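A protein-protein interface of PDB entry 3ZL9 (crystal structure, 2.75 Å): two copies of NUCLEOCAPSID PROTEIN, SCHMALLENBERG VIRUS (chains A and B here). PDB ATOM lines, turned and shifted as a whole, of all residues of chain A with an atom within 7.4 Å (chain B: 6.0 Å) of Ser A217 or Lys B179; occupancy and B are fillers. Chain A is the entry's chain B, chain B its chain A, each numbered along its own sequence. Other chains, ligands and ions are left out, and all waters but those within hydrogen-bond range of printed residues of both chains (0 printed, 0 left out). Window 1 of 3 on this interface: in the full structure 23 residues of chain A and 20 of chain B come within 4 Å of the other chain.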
ATOM      1  N   ALA A 128      25.628   2.918  10.374  1.00  0.00           N
ATOM      2  CA  ALA A 128      24.233   3.103  10.021  1.00  0.00           C
ATOM      3  C   ALA A 128      23.429   1.813  10.182  1.00  0.00           C
ATOM      4  O   ALA A 128      22.331   1.827  10.754  1.00  0.00           O
ATOM      5  CB  ALA A 128      24.121   3.601   8.595  1.00  0.00           C
ATOM      6  N   GLU A 129      23.974   0.702   9.689  1.00  0.00           N
ATOM      7  CA  GLU A 129      23.252  -0.578   9.717  1.00  0.00           C
ATOM      8  C   GLU A 129      23.011  -1.044  11.178  1.00  0.00           C
ATOM      9  O   GLU A 129      21.916  -1.466  11.513  1.00  0.00           O
ATOM     10  CB  GLU A 129      23.964  -1.662   8.885  1.00  0.00           C
ATOM     11  CG  GLU A 129      24.137  -1.346   7.402  1.00  0.00           C
ATOM     12  CD  GLU A 129      22.846  -1.296   6.560  1.00  0.00           C
ATOM     13  OE1 GLU A 129      21.856  -2.010   6.866  1.00  0.00           O
ATOM     14  OE2 GLU A 129      22.835  -0.557   5.543  1.00  0.00           O
ATOM     15  N   VAL A 130      24.016  -0.914  12.035  1.00  0.00           N
ATOM     16  CA  VAL A 130      23.887  -1.234  13.452  1.00  0.00           C
ATOM     17  C   VAL A 130      22.655  -0.575  14.078  1.00  0.00           C
ATOM     18  O   VAL A 130      21.984  -1.179  14.898  1.00  0.00           O
ATOM     19  CB  VAL A 130      25.162  -0.811  14.243  1.00  0.00           C
ATOM     20  CG1 VAL A 130      24.910  -0.771  15.747  1.00  0.00           C
ATOM     21  CG2 VAL A 130      26.306  -1.767  13.956  1.00  0.00           C
ATOM     22  N   LYS A 131      22.387   0.675  13.708  1.00  0.00           N
ATOM     23  CA  LYS A 131      21.249   1.435  14.257  1.00  0.00           C
ATOM     24  C   LYS A 131      20.009   1.340  13.377  1.00  0.00           C
ATOM     25  O   LYS A 131      19.069   2.115  13.547  1.00  0.00           O
ATOM     26  CB  LYS A 131      21.622   2.914  14.403  1.00  0.00           C
ATOM     27  CG  LYS A 131      22.858   3.167  15.257  1.00  0.00           C
ATOM     28  CD  LYS A 131      22.795   2.473  16.604  1.00  0.00           C
ATOM     29  CE  LYS A 131      24.027   2.826  17.419  1.00  0.00           C
ATOM     30  NZ  LYS A 131      24.303   1.866  18.528  1.00  0.00           N
ATOM     31  N   GLY A 132      20.016   0.408  12.426  1.00  0.00           N
ATOM     32  CA  GLY A 132      18.851   0.160  11.574  1.00  0.00           C
ATOM     33  C   GLY A 132      18.516   1.234  10.559  1.00  0.00           C
ATOM     34  O   GLY A 132      17.352   1.410  10.217  1.00  0.00           O
ATOM     35  N   CYS A 133      19.538   1.979  10.118  1.00  0.00           N
ATOM     36  CA  CYS A 133      19.402   3.017   9.090  1.00  0.00           C
ATOM     37  C   CYS A 133      19.874   2.425   7.770  1.00  0.00           C
ATOM     38  O   CYS A 133      20.847   1.680   7.738  1.00  0.00           O
ATOM     39  CB  CYS A 133      20.262   4.245   9.446  1.00  0.00           C
ATOM     40  SG  CYS A 133      20.130   5.618   8.260  1.00  0.00           S
ATOM     41  N   LEU A 212      14.725   5.909  14.064  1.00  0.00           N
ATOM     42  CA  LEU A 212      15.410   4.724  13.605  1.00  0.00           C
ATOM     43  C   LEU A 212      15.395   3.710  14.718  1.00  0.00           C
ATOM     44  O   LEU A 212      15.636   4.065  15.872  1.00  0.00           O
ATOM     45  CB  LEU A 212      16.869   5.034  13.247  1.00  0.00           C
ATOM     46  CG  LEU A 212      17.104   6.053  12.147  1.00  0.00           C
ATOM     47  CD1 LEU A 212      18.546   6.540  12.233  1.00  0.00           C
ATOM     48  CD2 LEU A 212      16.777   5.464  10.771  1.00  0.00           C
ATOM     49  N   ALA A 213      15.121   2.460  14.359  1.00  0.00           N
ATOM     50  CA  ALA A 213      15.287   1.340  15.263  1.00  0.00           C
ATOM     51  C   ALA A 213      16.696   1.381  15.837  1.00  0.00           C
ATOM     52  O   ALA A 213      17.604   0.728  15.335  1.00  0.00           O
ATOM     53  CB  ALA A 213      15.056   0.026  14.523  1.00  0.00           C
ATOM     54  N   TRP A 214      16.891   2.172  16.878  1.00  0.00           N
ATOM     55  CA  TRP A 214      18.221   2.326  17.449  1.00  0.00           C
ATOM     56  C   TRP A 214      18.634   0.991  18.122  1.00  0.00           C
ATOM     57  O   TRP A 214      19.356   0.185  17.521  1.00  0.00           O
ATOM     58  CB  TRP A 214      18.255   3.572  18.354  1.00  0.00           C
ATOM     59  CG  TRP A 214      19.608   4.064  18.622  1.00  0.00           C
ATOM     60  CD1 TRP A 214      20.484   3.606  19.565  1.00  0.00           C
ATOM     61  CD2 TRP A 214      20.260   5.138  17.951  1.00  0.00           C
ATOM     62  NE1 TRP A 214      21.650   4.334  19.516  1.00  0.00           N
ATOM     63  CE2 TRP A 214      21.538   5.280  18.531  1.00  0.00           C
ATOM     64  CE3 TRP A 214      19.890   5.997  16.903  1.00  0.00           C
ATOM     65  CZ2 TRP A 214      22.451   6.247  18.097  1.00  0.00           C
ATOM     66  CZ3 TRP A 214      20.791   6.949  16.477  1.00  0.00           C
ATOM     67  CH2 TRP A 214      22.060   7.066  17.073  1.00  0.00           C
ATOM     68  N   ALA A 215      18.126   0.712  19.316  1.00  0.00           N
ATOM     69  CA  ALA A 215      18.434  -0.575  19.961  1.00  0.00           C
ATOM     70  C   ALA A 215      17.580  -1.707  19.410  1.00  0.00           C
ATOM     71  O   ALA A 215      17.864  -2.858  19.663  1.00  0.00           O
ATOM     72  CB  ALA A 215      18.309  -0.498  21.482  1.00  0.00           C
ATOM     73  N   LYS A 216      16.548  -1.363  18.650  1.00  0.00           N
ATOM     74  CA  LYS A 216      15.580  -2.283  18.103  1.00  0.00           C
ATOM     75  C   LYS A 216      16.025  -2.882  16.765  1.00  0.00           C
ATOM     76  O   LYS A 216      15.332  -3.743  16.238  1.00  0.00           O
ATOM     77  CB  LYS A 216      14.290  -1.525  17.830  1.00  0.00           C
ATOM     78  CG  LYS A 216      13.621  -0.898  19.043  1.00  0.00           C
ATOM     79  CD  LYS A 216      12.419  -0.052  18.641  1.00  0.00           C
ATOM     80  CE  LYS A 216      12.698   1.440  18.597  1.00  0.00           C
ATOM     81  NZ  LYS A 216      11.499   2.225  18.170  1.00  0.00           N
ATOM     82  N   SER A 217      17.115  -2.379  16.167  1.00  0.00           N
ATOM     83  CA  SER A 217      17.616  -2.944  14.905  1.00  0.00           C
ATOM     84  C   SER A 217      17.820  -4.458  15.050  1.00  0.00           C
ATOM     85  O   SER A 217      18.533  -4.902  15.950  1.00  0.00           O
ATOM     86  CB  SER A 217      18.925  -2.288  14.495  1.00  0.00           C
ATOM     87  OG  SER A 217      19.157  -2.493  13.106  1.00  0.00           O
ATOM     88  N   GLY A 218      17.146  -5.241  14.202  1.00  0.00           N
ATOM     89  CA  GLY A 218      17.240  -6.708  14.239  1.00  0.00           C
ATOM     90  C   GLY A 218      16.151  -7.435  15.022  1.00  0.00           C
ATOM     91  O   GLY A 218      16.242  -8.642  15.238  1.00  0.00           O
ATOM     92  N   PHE A 219      15.150  -6.689  15.474  1.00  0.00           N
ATOM     93  CA  PHE A 219      13.923  -7.233  16.066  1.00  0.00           C
ATOM     94  C   PHE A 219      12.768  -6.762  15.195  1.00  0.00           C
ATOM     95  O   PHE A 219      12.515  -5.564  15.107  1.00  0.00           O
ATOM     96  CB  PHE A 219      13.664  -6.673  17.464  1.00  0.00           C
ATOM     97  CG  PHE A 219      14.661  -7.088  18.503  1.00  0.00           C
ATOM     98  CD1 PHE A 219      14.565  -8.320  19.121  1.00  0.00           C
ATOM     99  CD2 PHE A 219      15.651  -6.209  18.928  1.00  0.00           C
ATOM    100  CE1 PHE A 219      15.468  -8.687  20.107  1.00  0.00           C
ATOM    101  CE2 PHE A 219      16.562  -6.568  19.912  1.00  0.00           C
ATOM    102  CZ  PHE A 219      16.467  -7.813  20.505  1.00  0.00           C
ATOM    103  N   SER A 220      12.044  -7.678  14.573  1.00  0.00           N
ATOM    104  CA  SER A 220      10.894  -7.283  13.774  1.00  0.00           C
ATOM    105  C   SER A 220       9.882  -6.579  14.669  1.00  0.00           C
ATOM    106  O   SER A 220       9.891  -6.765  15.892  1.00  0.00           O
ATOM    107  CB  SER A 220      10.230  -8.504  13.166  1.00  0.00           C
ATOM    108  OG  SER A 220       9.635  -9.291  14.193  1.00  0.00           O
ATOM    109  N   ALA A 223       8.161  -9.007  16.862  1.00  0.00           N
ATOM    110  CA  ALA A 223       9.002  -9.481  17.952  1.00  0.00           C
ATOM    111  C   ALA A 223       8.962  -8.521  19.135  1.00  0.00           C
ATOM    112  O   ALA A 223       9.064  -8.940  20.283  1.00  0.00           O
ATOM    113  CB  ALA A 223      10.435  -9.649  17.467  1.00  0.00           C
ATOM    114  N   ARG A 224       8.835  -7.227  18.865  1.00  0.00           N
ATOM    115  CA  ARG A 224       8.837  -6.224  19.939  1.00  0.00           C
ATOM    116  C   ARG A 224       7.526  -6.294  20.702  1.00  0.00           C
ATOM    117  O   ARG A 224       7.518  -6.276  21.942  1.00  0.00           O
ATOM    118  CB  ARG A 224       9.016  -4.838  19.376  1.00  0.00           C
ATOM    119  CG  ARG A 224      10.400  -4.217  19.526  1.00  0.00           C
ATOM    120  CD  ARG A 224      10.527  -3.036  18.539  1.00  0.00           C
ATOM    121  NE  ARG A 224      10.858  -3.489  17.185  1.00  0.00           N
ATOM    122  CZ  ARG A 224      10.668  -2.778  16.073  1.00  0.00           C
ATOM    123  NH1 ARG A 224      10.109  -1.567  16.110  1.00  0.00           N
ATOM    124  NH2 ARG A 224      11.023  -3.286  14.899  1.00  0.00           N
ATOM    125  N   ILE A 234      12.260  -2.543  24.367  1.00  0.00           N
ATOM    126  CA  ILE A 234      13.486  -2.321  23.619  1.00  0.00           C
ATOM    127  C   ILE A 234      13.724  -0.828  23.450  1.00  0.00           C
ATOM    128  O   ILE A 234      12.839  -0.107  23.008  1.00  0.00           O
ATOM    129  CB  ILE A 234      13.424  -3.003  22.232  1.00  0.00           C
ATOM    130  CG1 ILE A 234      12.821  -4.420  22.359  1.00  0.00           C
ATOM    131  CG2 ILE A 234      14.815  -2.956  21.576  1.00  0.00           C
ATOM    132  CD1 ILE A 234      13.793  -5.483  22.780  1.00  0.00           C
ATOM    133  N   VAL B 175      20.026  -8.234  25.841  1.00  0.00           N
ATOM    134  CA  VAL B 175      18.825  -8.504  25.056  1.00  0.00           C
ATOM    135  C   VAL B 175      19.141  -8.988  23.636  1.00  0.00           C
ATOM    136  O   VAL B 175      18.370  -9.742  23.037  1.00  0.00           O
ATOM    137  CB  VAL B 175      17.955  -7.231  24.923  1.00  0.00           C
ATOM    138  CG1 VAL B 175      16.512  -7.610  24.611  1.00  0.00           C
ATOM    139  CG2 VAL B 175      18.025  -6.378  26.183  1.00  0.00           C
ATOM    140  N   ASN B 176      20.266  -8.533  23.097  1.00  0.00           N
ATOM    141  CA  ASN B 176      20.642  -8.868  21.733  1.00  0.00           C
ATOM    142  C   ASN B 176      20.872 -10.349  21.503  1.00  0.00           C
ATOM    143  O   ASN B 176      20.830 -10.795  20.359  1.00  0.00           O
ATOM    144  CB  ASN B 176      21.911  -8.108  21.330  1.00  0.00           C
ATOM    145  CG  ASN B 176      21.678  -6.618  21.166  1.00  0.00           C
ATOM    146  OD1 ASN B 176      20.540  -6.132  21.247  1.00  0.00           O
ATOM    147  ND2 ASN B 176      22.763  -5.883  20.904  1.00  0.00           N
ATOM    148  N   PHE B 177      21.130 -11.103  22.575  1.00  0.00           N
ATOM    149  CA  PHE B 177      21.302 -12.549  22.469  1.00  0.00           C
ATOM    150  C   PHE B 177      19.977 -13.270  22.215  1.00  0.00           C
ATOM    151  O   PHE B 177      19.958 -14.491  22.007  1.00  0.00           O
ATOM    152  CB  PHE B 177      21.979 -13.135  23.727  1.00  0.00           C
ATOM    153  CG  PHE B 177      23.374 -12.625  23.977  1.00  0.00           C
ATOM    154  CD1 PHE B 177      24.300 -12.515  22.939  1.00  0.00           C
ATOM    155  CD2 PHE B 177      23.774 -12.289  25.252  1.00  0.00           C
ATOM    156  CE1 PHE B 177      25.577 -12.036  23.174  1.00  0.00           C
ATOM    157  CE2 PHE B 177      25.057 -11.820  25.500  1.00  0.00           C
ATOM    158  CZ  PHE B 177      25.957 -11.691  24.458  1.00  0.00           C
ATOM    159  N   MET B 178      18.879 -12.522  22.231  1.00  0.00           N
ATOM    160  CA  MET B 178      17.566 -13.080  21.912  1.00  0.00           C
ATOM    161  C   MET B 178      17.142 -12.871  20.465  1.00  0.00           C
ATOM    162  O   MET B 178      16.141 -13.448  20.024  1.00  0.00           O
ATOM    163  CB  MET B 178      16.514 -12.449  22.791  1.00  0.00           C
ATOM    164  CG  MET B 178      16.503 -13.007  24.189  1.00  0.00           C
ATOM    165  SD  MET B 178      14.865 -12.779  24.865  1.00  0.00           S
ATOM    166  CE  MET B 178      13.925 -13.992  23.938  1.00  0.00           C
ATOM    167  N   LYS B 179      17.893 -12.050  19.732  1.00  0.00           N
ATOM    168  CA  LYS B 179      17.610 -11.806  18.317  1.00  0.00           C
ATOM    169  C   LYS B 179      17.403 -13.132  17.576  1.00  0.00           C
ATOM    170  O   LYS B 179      16.356 -13.350  16.998  1.00  0.00           O
ATOM    171  CB  LYS B 179      18.705 -10.938  17.694  1.00  0.00           C
ATOM    172  CG  LYS B 179      18.548  -9.479  18.111  1.00  0.00           C
ATOM    173  CD  LYS B 179      19.802  -8.619  17.977  1.00  0.00           C
ATOM    174  CE  LYS B 179      20.081  -8.248  16.532  1.00  0.00           C
ATOM    175  NZ  LYS B 179      20.707  -6.907  16.411  1.00  0.00           N
ATOM    176  N   LYS B 180      18.348 -14.050  17.716  1.00  0.00           N
ATOM    177  CA  LYS B 180      18.297 -15.346  17.044  1.00  0.00           C
ATOM    178  C   LYS B 180      17.028 -16.145  17.376  1.00  0.00           C
ATOM    179  O   LYS B 180      16.255 -16.512  16.486  1.00  0.00           O
ATOM    180  CB  LYS B 180      19.544 -16.175  17.409  1.00  0.00           C
ATOM    181  CG  LYS B 180      19.923 -17.255  16.406  1.00  0.00           C
ATOM    182  CD  LYS B 180      20.851 -18.303  17.026  1.00  0.00           C
ATOM    183  CE  LYS B 180      21.555 -19.152  15.970  1.00  0.00           C
ATOM    184  NZ  LYS B 180      20.601 -19.794  15.013  1.00  0.00           N
ATOM    185  N   VAL B 181      16.817 -16.416  18.655  1.00  0.00           N
ATOM    186  CA  VAL B 181      15.678 -17.260  19.102  1.00  0.00           C
ATOM    187  C   VAL B 181      14.353 -16.793  18.512  1.00  0.00           C
ATOM    188  O   VAL B 181      13.532 -17.604  18.134  1.00  0.00           O
ATOM    189  CB  VAL B 181      15.484 -17.259  20.640  1.00  0.00           C
ATOM    190  CG1 VAL B 181      14.591 -18.419  21.048  1.00  0.00           C
ATOM    191  CG2 VAL B 181      16.815 -17.340  21.373  1.00  0.00           C
ATOM    192  N   LEU B 182      14.161 -15.479  18.455  1.00  0.00           N
ATOM    193  CA  LEU B 182      12.925 -14.874  17.971  1.00  0.00           C
ATOM    194  C   LEU B 182      12.785 -14.944  16.462  1.00  0.00           C
ATOM    195  O   LEU B 182      11.841 -14.375  15.900  1.00  0.00           O
ATOM    196  CB  LEU B 182      12.884 -13.424  18.384  1.00  0.00           C
ATOM    197  CG  LEU B 182      12.908 -13.190  19.891  1.00  0.00           C
ATOM    198  CD1 LEU B 182      13.360 -11.774  20.222  1.00  0.00           C
ATOM    199  CD2 LEU B 182      11.533 -13.475  20.486  1.00  0.00           C
ATOM    200  N   ARG B 183      13.733 -15.624  15.795  1.00  0.00           N
ATOM    201  CA  ARG B 183      13.614 -15.913  14.356  1.00  0.00           C
ATOM    202  C   ARG B 183      13.337 -17.391  14.089  1.00  0.00           C
ATOM    203  O   ARG B 183      13.240 -17.807  12.950  1.00  0.00           O
ATOM    204  CB  ARG B 183      14.887 -15.492  13.639  1.00  0.00           C
ATOM    205  CG  ARG B 183      15.259 -14.026  13.834  1.00  0.00           C
ATOM    206  CD  ARG B 183      16.373 -13.646  12.879  1.00  0.00           C
ATOM    207  NE  ARG B 183      16.751 -12.237  13.016  1.00  0.00           N
ATOM    208  CZ  ARG B 183      17.904 -11.781  13.519  1.00  0.00           C
ATOM    209  NH1 ARG B 183      18.863 -12.600  13.974  1.00  0.00           N
ATOM    210  NH2 ARG B 183      18.111 -10.473  13.558  1.00  0.00           N
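The guanidinium group of Arg B183 is in hydrogen-bond range of the backbone carbonyl oxygen of Gly A218 (3.1 Å). NZ of Lys B179 is in hydrogen-bond range of O of Ser A217.
The guanidinium group (NH2) of Arg A224 lies within hydrogen-bond range of the backbone carbonyl oxygen (O) of Phe A219 (2.7 Å). The backbone NH of Gly A132 lies close to the side-chain hydroxyl of Ser A217, at 3.1 Å. The backbone carbonyl oxygen (O) of Glu A129 sits at hydrogen-bond distance from the side-chain hydroxyl (OG) of Ser A217, 3.3 Å away.
Gly A218 touches Lys B179 (O to CG, 3.8 Å). Phe A219 touches Val B175 (CZ to O, 3.7 Å). Phe A219 touches Lys B179. CD1 of Leu B182 touches CE1 of Phe A219 (3.7 Å). Val B175 touches Ile A234.
Ser A217 touches just one residue of chain B: Lys B179. Printed residues of chain B within 4 Å of Phe A219: Val B175, Lys B179 and Leu B182. Arg A224 touches none of the printed residues of chain B. Of the printed residues of chain A, Lys B179 touches Ser A217, Gly A218 and Phe A219. Printed residues of chain A within 4 Å of Leu B182: Phe A219 (3.7 Å). Printed residues of chain A within 4 Å of Arg B183: Gly A218 (3.1 Å). The nearest residue of chain A that does not touch Lys B179 is Ala A215 (5.9 Å). The nearest printed residue of chain B that does not touch Ile A234 is Asn B176 (6.6 Å).
Printed residues of chain A that touch a printed residue of chain B: Ser A217, Gly A218, Phe A219 and Ile A234. Along chain A the printed residues that touch a printed residue of chain B span positions 217 to 234. Of the 9 printed residues of chain B, 4 touch a printed residue of chain A. Among the printed residues, no Asp or Glu carboxylate lies within 4 Å of a Lys or Arg side-chain nitrogen of the other chain.
No position is printed for both chains. Of the 7 pairs that touch across the chains among the printed residues, none has its exchanged pair printed and touching as well.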
